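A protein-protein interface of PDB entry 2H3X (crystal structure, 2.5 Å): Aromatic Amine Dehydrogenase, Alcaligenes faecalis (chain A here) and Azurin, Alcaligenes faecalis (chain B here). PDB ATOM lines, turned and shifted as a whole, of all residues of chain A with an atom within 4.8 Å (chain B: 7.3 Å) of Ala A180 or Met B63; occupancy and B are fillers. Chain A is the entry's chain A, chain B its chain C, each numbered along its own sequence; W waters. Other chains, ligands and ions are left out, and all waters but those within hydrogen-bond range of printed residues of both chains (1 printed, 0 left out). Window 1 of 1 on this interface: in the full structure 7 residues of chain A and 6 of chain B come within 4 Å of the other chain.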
ATOM      1  N   THR A 160     -29.638  -7.179  15.866  1.00  0.00           N
ATOM      2  CA  THR A 160     -30.655  -7.269  14.831  1.00  0.00           C
ATOM      3  C   THR A 160     -31.690  -8.365  15.050  1.00  0.00           C
ATOM      4  O   THR A 160     -31.418  -9.396  15.669  1.00  0.00           O
ATOM      5  CB  THR A 160     -30.012  -7.461  13.434  1.00  0.00           C
ATOM      6  OG1 THR A 160     -29.429  -8.767  13.344  1.00  0.00           O
ATOM      7  CG2 THR A 160     -28.931  -6.416  13.201  1.00  0.00           C
ATOM      8  N   THR A 177     -35.931 -13.130  16.808  1.00  0.00           N
ATOM      9  CA  THR A 177     -34.585 -12.924  17.317  1.00  0.00           C
ATOM     10  C   THR A 177     -33.598 -13.932  16.745  1.00  0.00           C
ATOM     11  O   THR A 177     -32.393 -13.780  16.889  1.00  0.00           O
ATOM     12  CB  THR A 177     -34.571 -13.028  18.839  1.00  0.00           C
ATOM     13  OG1 THR A 177     -35.035 -14.329  19.222  1.00  0.00           O
ATOM     14  CG2 THR A 177     -35.480 -11.972  19.446  1.00  0.00           C
ATOM     15  N   ALA A 178     -34.111 -14.965  16.092  1.00  0.00           N
ATOM     16  CA  ALA A 178     -33.249 -15.975  15.498  1.00  0.00           C
ATOM     17  C   ALA A 178     -32.449 -15.359  14.353  1.00  0.00           C
ATOM     18  O   ALA A 178     -31.455 -15.926  13.887  1.00  0.00           O
ATOM     19  CB  ALA A 178     -34.088 -17.129  14.981  1.00  0.00           C
ATOM     20  N   ALA A 179     -32.891 -14.190  13.904  1.00  0.00           N
ATOM     21  CA  ALA A 179     -32.237 -13.500  12.801  1.00  0.00           C
ATOM     22  C   ALA A 179     -31.031 -12.670  13.230  1.00  0.00           C
ATOM     23  O   ALA A 179     -30.424 -11.993  12.403  1.00  0.00           O
ATOM     24  CB  ALA A 179     -33.245 -12.618  12.072  1.00  0.00           C
ATOM     25  N   ALA A 180     -30.677 -12.723  14.509  1.00  0.00           N
ATOM     26  CA  ALA A 180     -29.536 -11.958  14.993  1.00  0.00           C
ATOM     27  C   ALA A 180     -28.309 -12.306  14.163  1.00  0.00           C
ATOM     28  O   ALA A 180     -28.028 -13.479  13.916  1.00  0.00           O
ATOM     29  CB  ALA A 180     -29.276 -12.254  16.475  1.00  0.00           C
ATOM     30  N   GLY A 181     -27.586 -11.275  13.738  1.00  0.00           N
ATOM     31  CA  GLY A 181     -26.400 -11.477  12.931  1.00  0.00           C
ATOM     32  C   GLY A 181     -26.746 -11.569  11.460  1.00  0.00           C
ATOM     33  O   GLY A 181     -25.864 -11.775  10.622  1.00  0.00           O
ATOM     34  N   CYS A 182     -28.032 -11.424  11.145  1.00  0.00           N
ATOM     35  CA  CYS A 182     -28.498 -11.479   9.762  1.00  0.00           C
ATOM     36  C   CYS A 182     -29.027 -10.098   9.369  1.00  0.00           C
ATOM     37  O   CYS A 182     -29.172  -9.220  10.227  1.00  0.00           O
ATOM     38  CB  CYS A 182     -29.590 -12.545   9.603  1.00  0.00           C
ATOM     39  SG  CYS A 182     -29.091 -14.197  10.202  1.00  0.00           S
ATOM     40  N   CYS A 199     -27.059 -13.816   6.249  1.00  0.00           N
ATOM     41  CA  CYS A 199     -26.389 -13.818   7.547  1.00  0.00           C
ATOM     42  C   CYS A 199     -24.876 -13.689   7.466  1.00  0.00           C
ATOM     43  O   CYS A 199     -24.267 -13.926   6.423  1.00  0.00           O
ATOM     44  CB  CYS A 199     -26.781 -15.063   8.348  1.00  0.00           C
ATOM     45  SG  CYS A 199     -28.592 -15.267   8.532  1.00  0.00           S
ATOM     46  N   GLY A 200     -24.279 -13.277   8.583  1.00  0.00           N
ATOM     47  CA  GLY A 200     -22.840 -13.076   8.655  1.00  0.00           C
ATOM     48  C   GLY A 200     -21.969 -14.298   8.422  1.00  0.00           C
ATOM     49  O   GLY A 200     -20.746 -14.189   8.404  1.00  0.00           O
ATOM     50  N   ASP A 201     -22.580 -15.466   8.262  1.00  0.00           N
ATOM     51  CA  ASP A 201     -21.814 -16.682   8.009  1.00  0.00           C
ATOM     52  C   ASP A 201     -21.762 -16.927   6.503  1.00  0.00           C
ATOM     53  O   ASP A 201     -21.218 -17.929   6.046  1.00  0.00           O
ATOM     54  CB  ASP A 201     -22.459 -17.887   8.702  1.00  0.00           C
ATOM     55  CG  ASP A 201     -23.801 -18.263   8.098  1.00  0.00           C
ATOM     56  OD1 ASP A 201     -24.624 -17.357   7.834  1.00  0.00           O
ATOM     57  OD2 ASP A 201     -24.038 -19.470   7.898  1.00  0.00           O
ATOM     58  N   ARG A 220     -31.464 -23.136   7.787  1.00  0.00           N
ATOM     59  CA  ARG A 220     -30.319 -22.392   7.285  1.00  0.00           C
ATOM     60  C   ARG A 220     -29.734 -23.132   6.092  1.00  0.00           C
ATOM     61  O   ARG A 220     -29.699 -24.359   6.072  1.00  0.00           O
ATOM     62  CB  ARG A 220     -29.243 -22.252   8.359  1.00  0.00           C
ATOM     63  CG  ARG A 220     -29.522 -21.212   9.417  1.00  0.00           C
ATOM     64  CD  ARG A 220     -28.286 -20.986  10.276  1.00  0.00           C
ATOM     65  NE  ARG A 220     -28.180 -19.591  10.703  1.00  0.00           N
ATOM     66  CZ  ARG A 220     -28.907 -19.036  11.669  1.00  0.00           C
ATOM     67  NH1 ARG A 220     -29.802 -19.754  12.331  1.00  0.00           N
ATOM     68  NH2 ARG A 220     -28.750 -17.754  11.959  1.00  0.00           N
ATOM     69  N   ALA B  41     -29.784  -7.914  25.426  1.00  0.00           N
ATOM     70  CA  ALA B  41     -30.449  -8.144  24.150  1.00  0.00           C
ATOM     71  C   ALA B  41     -29.962  -7.201  23.052  1.00  0.00           C
ATOM     72  O   ALA B  41     -30.146  -7.477  21.868  1.00  0.00           O
ATOM     73  CB  ALA B  41     -31.962  -8.004  24.320  1.00  0.00           C
ATOM     74  N   ALA B  57     -14.126 -18.712  13.130  1.00  0.00           N
ATOM     75  CA  ALA B  57     -15.002 -19.870  13.020  1.00  0.00           C
ATOM     76  C   ALA B  57     -15.951 -20.042  14.205  1.00  0.00           C
ATOM     77  O   ALA B  57     -17.123 -20.367  14.020  1.00  0.00           O
ATOM     78  CB  ALA B  57     -14.163 -21.128  12.839  1.00  0.00           C
ATOM     79  N   VAL B  58     -15.449 -19.840  15.418  1.00  0.00           N
ATOM     80  CA  VAL B  58     -16.287 -19.994  16.602  1.00  0.00           C
ATOM     81  C   VAL B  58     -17.360 -18.915  16.708  1.00  0.00           C
ATOM     82  O   VAL B  58     -18.497 -19.207  17.068  1.00  0.00           O
ATOM     83  CB  VAL B  58     -15.441 -20.003  17.898  1.00  0.00           C
ATOM     84  CG1 VAL B  58     -16.348 -19.976  19.112  1.00  0.00           C
ATOM     85  CG2 VAL B  58     -14.575 -21.255  17.939  1.00  0.00           C
ATOM     86  N   ALA B  59     -17.001 -17.674  16.392  1.00  0.00           N
ATOM     87  CA  ALA B  59     -17.953 -16.566  16.457  1.00  0.00           C
ATOM     88  C   ALA B  59     -19.085 -16.762  15.451  1.00  0.00           C
ATOM     89  O   ALA B  59     -20.242 -16.466  15.738  1.00  0.00           O
ATOM     90  CB  ALA B  59     -17.241 -15.248  16.190  1.00  0.00           C
ATOM     91  N   THR B  60     -18.742 -17.261  14.273  1.00  0.00           N
ATOM     92  CA  THR B  60     -19.722 -17.502  13.226  1.00  0.00           C
ATOM     93  C   THR B  60     -20.675 -18.617  13.656  1.00  0.00           C
ATOM     94  O   THR B  60     -21.888 -18.520  13.459  1.00  0.00           O
ATOM     95  CB  THR B  60     -19.029 -17.913  11.915  1.00  0.00           C
ATOM     96  OG1 THR B  60     -17.990 -16.976  11.611  1.00  0.00           O
ATOM     97  CG2 THR B  60     -20.023 -17.937  10.770  1.00  0.00           C
ATOM     98  N   ASP B  61     -20.115 -19.675  14.234  1.00  0.00           N
ATOM     99  CA  ASP B  61     -20.909 -20.804  14.702  1.00  0.00           C
ATOM    100  C   ASP B  61     -21.668 -20.417  15.961  1.00  0.00           C
ATOM    101  O   ASP B  61     -22.747 -20.945  16.233  1.00  0.00           O
ATOM    102  CB  ASP B  61     -20.008 -22.011  14.990  1.00  0.00           C
ATOM    103  CG  ASP B  61     -19.700 -22.824  13.746  1.00  0.00           C
ATOM    104  OD1 ASP B  61     -18.824 -23.711  13.810  1.00  0.00           O
ATOM    105  OD2 ASP B  61     -20.344 -22.584  12.705  1.00  0.00           O
ATOM    106  N   GLY B  62     -21.097 -19.490  16.727  1.00  0.00           N
ATOM    107  CA  GLY B  62     -21.738 -19.041  17.952  1.00  0.00           C
ATOM    108  C   GLY B  62     -22.950 -18.187  17.639  1.00  0.00           C
ATOM    109  O   GLY B  62     -23.960 -18.222  18.339  1.00  0.00           O
ATOM    110  N   MET B  63     -22.839 -17.411  16.570  1.00  0.00           N
ATOM    111  CA  MET B  63     -23.920 -16.548  16.139  1.00  0.00           C
ATOM    112  C   MET B  63     -25.152 -17.396  15.852  1.00  0.00           C
ATOM    113  O   MET B  63     -26.272 -17.001  16.178  1.00  0.00           O
ATOM    114  CB  MET B  63     -23.502 -15.798  14.877  1.00  0.00           C
ATOM    115  CG  MET B  63     -24.591 -14.937  14.270  1.00  0.00           C
ATOM    116  SD  MET B  63     -24.505 -14.964  12.479  1.00  0.00           S
ATOM    117  CE  MET B  63     -25.708 -16.187  12.111  1.00  0.00           C
ATOM    118  N   LYS B  64     -24.935 -18.562  15.246  1.00  0.00           N
ATOM    119  CA  LYS B  64     -26.027 -19.469  14.901  1.00  0.00           C
ATOM    120  C   LYS B  64     -26.589 -20.185  16.127  1.00  0.00           C
ATOM    121  O   LYS B  64     -27.700 -20.718  16.088  1.00  0.00           O
ATOM    122  CB  LYS B  64     -25.567 -20.531  13.892  1.00  0.00           C
ATOM    123  CG  LYS B  64     -24.872 -20.023  12.639  1.00  0.00           C
ATOM    124  CD  LYS B  64     -24.798 -21.149  11.613  1.00  0.00           C
ATOM    125  CE  LYS B  64     -23.712 -20.929  10.567  1.00  0.00           C
ATOM    126  NZ  LYS B  64     -22.344 -21.160  11.116  1.00  0.00           N
ATOM    127  N   ALA B  65     -25.816 -20.210  17.209  1.00  0.00           N
ATOM    128  CA  ALA B  65     -26.251 -20.876  18.431  1.00  0.00           C
ATOM    129  C   ALA B  65     -27.404 -20.127  19.090  1.00  0.00           C
ATOM    130  O   ALA B  65     -28.334 -20.742  19.615  1.00  0.00           O
ATOM    131  CB  ALA B  65     -25.083 -21.003  19.407  1.00  0.00           C
ATOM    132  N   GLY B  66     -27.338 -18.799  19.055  1.00  0.00           N
ATOM    133  CA  GLY B  66     -28.387 -17.990  19.653  1.00  0.00           C
ATOM    134  C   GLY B  66     -28.052 -17.516  21.059  1.00  0.00           C
ATOM    135  O   GLY B  66     -27.145 -18.048  21.706  1.00  0.00           O
ATOM    136  N   LEU B  67     -28.783 -16.512  21.535  1.00  0.00           N
ATOM    137  CA  LEU B  67     -28.551 -15.983  22.866  1.00  0.00           C
ATOM    138  C   LEU B  67     -28.781 -17.064  23.919  1.00  0.00           C
ATOM    139  O   LEU B  67     -28.186 -17.026  24.991  1.00  0.00           O
ATOM    140  CB  LEU B  67     -29.469 -14.785  23.129  1.00  0.00           C
ATOM    141  CG  LEU B  67     -29.374 -14.109  24.503  1.00  0.00           C
ATOM    142  CD1 LEU B  67     -27.976 -13.551  24.731  1.00  0.00           C
ATOM    143  CD2 LEU B  67     -30.410 -13.004  24.585  1.00  0.00           C
ATOM    144  N   ASP B  70     -25.584 -18.530  24.779  1.00  0.00           N
ATOM    145  CA  ASP B  70     -24.586 -17.492  24.988  1.00  0.00           C
ATOM    146  C   ASP B  70     -23.704 -17.265  23.769  1.00  0.00           C
ATOM    147  O   ASP B  70     -22.520 -16.965  23.892  1.00  0.00           O
ATOM    148  CB  ASP B  70     -23.740 -17.826  26.216  1.00  0.00           C
ATOM    149  CG  ASP B  70     -24.551 -17.798  27.502  1.00  0.00           C
ATOM    150  OD1 ASP B  70     -25.106 -16.728  27.838  1.00  0.00           O
ATOM    151  OD2 ASP B  70     -24.640 -18.845  28.177  1.00  0.00           O
ATOM    152  N   TYR B  71     -24.311 -17.391  22.592  1.00  0.00           N
ATOM    153  CA  TYR B  71     -23.622 -17.208  21.318  1.00  0.00           C
ATOM    154  C   TYR B  71     -22.344 -18.022  21.184  1.00  0.00           C
ATOM    155  O   TYR B  71     -21.299 -17.517  20.772  1.00  0.00           O
ATOM    156  CB  TYR B  71     -23.346 -15.724  21.079  1.00  0.00           C
ATOM    157  CG  TYR B  71     -24.595 -14.973  20.690  1.00  0.00           C
ATOM    158  CD1 TYR B  71     -25.300 -15.320  19.537  1.00  0.00           C
ATOM    159  CD2 TYR B  71     -25.103 -13.948  21.490  1.00  0.00           C
ATOM    160  CE1 TYR B  71     -26.481 -14.673  19.192  1.00  0.00           C
ATOM    161  CE2 TYR B  71     -26.290 -13.290  21.149  1.00  0.00           C
ATOM    162  CZ  TYR B  71     -26.971 -13.661  20.001  1.00  0.00           C
ATOM    163  OH  TYR B  71     -28.143 -13.032  19.668  1.00  0.00           O
ATOM    164  N   VAL B  72     -22.457 -19.300  21.533  1.00  0.00           N
ATOM    165  CA  VAL B  72     -21.362 -20.254  21.462  1.00  0.00           C
ATOM    166  C   VAL B  72     -22.008 -21.599  21.176  1.00  0.00           C
ATOM    167  O   VAL B  72     -22.834 -22.073  21.958  1.00  0.00           O
ATOM    168  CB  VAL B  72     -20.591 -20.341  22.801  1.00  0.00           C
ATOM    169  CG1 VAL B  72     -19.627 -21.513  22.771  1.00  0.00           C
ATOM    170  CG2 VAL B  72     -19.834 -19.050  23.053  1.00  0.00           C
ATOM    171  N   LYS B  73     -21.654 -22.212  20.052  1.00  0.00           N
ATOM    172  CA  LYS B  73     -22.231 -23.503  19.724  1.00  0.00           C
ATOM    173  C   LYS B  73     -22.068 -24.433  20.914  1.00  0.00           C
ATOM    174  O   LYS B  73     -20.966 -24.591  21.447  1.00  0.00           O
ATOM    175  CB  LYS B  73     -21.555 -24.112  18.498  1.00  0.00           C
ATOM    176  CG  LYS B  73     -22.166 -25.446  18.082  1.00  0.00           C
ATOM    177  CD  LYS B  73     -21.685 -25.905  16.709  1.00  0.00           C
ATOM    178  CE  LYS B  73     -20.184 -26.156  16.684  1.00  0.00           C
ATOM    179  NZ  LYS B  73     -19.738 -26.637  15.345  1.00  0.00           N
ATOM    180  N   SER B 112     -18.316 -13.275  21.445  1.00  0.00           N
ATOM    181  CA  SER B 112     -18.963 -13.894  20.294  1.00  0.00           C
ATOM    182  C   SER B 112     -20.332 -13.298  19.987  1.00  0.00           C
ATOM    183  O   SER B 112     -20.984 -13.708  19.025  1.00  0.00           O
ATOM    184  CB  SER B 112     -19.086 -15.403  20.503  1.00  0.00           C
ATOM    185  OG  SER B 112     -19.753 -15.702  21.714  1.00  0.00           O
ATOM    186  N   PHE B 113     -20.768 -12.339  20.802  1.00  0.00           N
ATOM    187  CA  PHE B 113     -22.052 -11.672  20.584  1.00  0.00           C
ATOM    188  C   PHE B 113     -21.978 -11.098  19.170  1.00  0.00           C
ATOM    189  O   PHE B 113     -21.073 -10.331  18.852  1.00  0.00           O
ATOM    190  CB  PHE B 113     -22.253 -10.553  21.611  1.00  0.00           C
ATOM    191  CG  PHE B 113     -23.643  -9.975  21.622  1.00  0.00           C
ATOM    192  CD1 PHE B 113     -24.058  -9.100  20.629  1.00  0.00           C
ATOM    193  CD2 PHE B 113     -24.540 -10.311  22.631  1.00  0.00           C
ATOM    194  CE1 PHE B 113     -25.349  -8.565  20.641  1.00  0.00           C
ATOM    195  CE2 PHE B 113     -25.831  -9.784  22.649  1.00  0.00           C
ATOM    196  CZ  PHE B 113     -26.236  -8.910  21.652  1.00  0.00           C
ATOM    197  N   PRO B 114     -22.936 -11.465  18.309  1.00  0.00           N
ATOM    198  CA  PRO B 114     -23.025 -11.036  16.912  1.00  0.00           C
ATOM    199  C   PRO B 114     -22.364  -9.712  16.518  1.00  0.00           C
ATOM    200  O   PRO B 114     -22.833  -8.624  16.871  1.00  0.00           O
ATOM    201  CB  PRO B 114     -24.523 -11.058  16.656  1.00  0.00           C
ATOM    202  CG  PRO B 114     -24.928 -12.278  17.407  1.00  0.00           C
ATOM    203  CD  PRO B 114     -24.205 -12.089  18.726  1.00  0.00           C
ATOM    204  N   GLY B 115     -21.261  -9.833  15.784  1.00  0.00           N
ATOM    205  CA  GLY B 115     -20.534  -8.674  15.301  1.00  0.00           C
ATOM    206  C   GLY B 115     -19.488  -8.019  16.188  1.00  0.00           C
ATOM    207  O   GLY B 115     -18.743  -7.167  15.706  1.00  0.00           O
HETATM  208  O   HOH W   1     -22.088 -21.600   7.655  1.00  0.00           O
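The side-chain hydroxyl (OG1) of Thr A160 sits at hydrogen-bond distance from the backbone NH (N) of Gly A181, 3.1 Å away. The backbone NH (N) of Gly A200 lies within hydrogen-bond range of the backbone carbonyl oxygen (O) of Gly A181, 3.0 Å away. OD2 of Asp B61 lies within salt-bridge range of NZ of Lys B64 (2.9 Å). The backbone NH of Tyr B71 lies within hydrogen-bond range of the backbone carbonyl oxygen of Gly B66 (3.0 Å). The backbone carbonyl oxygen (O) of Tyr B71 lies within hydrogen-bond range of the side-chain hydroxyl (OG) of Ser B112, 2.6 Å away. SG of Cys A182 is disulfide-bonded to SG of Cys A199.
CG of Met B63 touches O of Ala A180, at 3.8 Å. Ala A180 touches Tyr B71. SD of Met B63 touches O of Gly A181, at 3.9 Å. Asp A201 touches Thr B60 (CB to CG2, 3.2 Å). Asp A201 touches Lys B64 (OD2 to CE, 3.1 Å). Met B63 touches Arg A220 (CE to NH2, 3.4 Å). CD of Arg A220 touches CD of Lys B64, 3.7 Å away.
Of chain B, only Met B63 (3.8 Å) and Tyr B71 (3.5 Å) come within 4 Å of Ala A180. Of the printed residues of chain B, Asp A201 touches Thr B60 (3.2 Å) and Lys B64 (3.1 Å). Printed residues of chain A within 4 Å of Thr B60: Asp A201 (3.2 Å). Of the printed residues of chain A, Met B63 touches Ala A180, Gly A181 and Arg A220. Printed residues of chain A within 4 Å of Tyr B71: Ala A180 (3.5 Å). The nearest residue of chain A that does not touch Met B63 is Cys A199 (4.1 Å).
Of the 11 printed residues of chain A, 4 touch a printed residue of chain B. Hydrophobic or aromatic side chains of chain A that line the printed part of chain B: Ala A180. Among the printed residues, 7 pairs touch across the chains.
Water W1 bridges the side-chain carboxylate (OD2) of Asp A201 and the side-chain amino group (NZ) of Lys B64.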
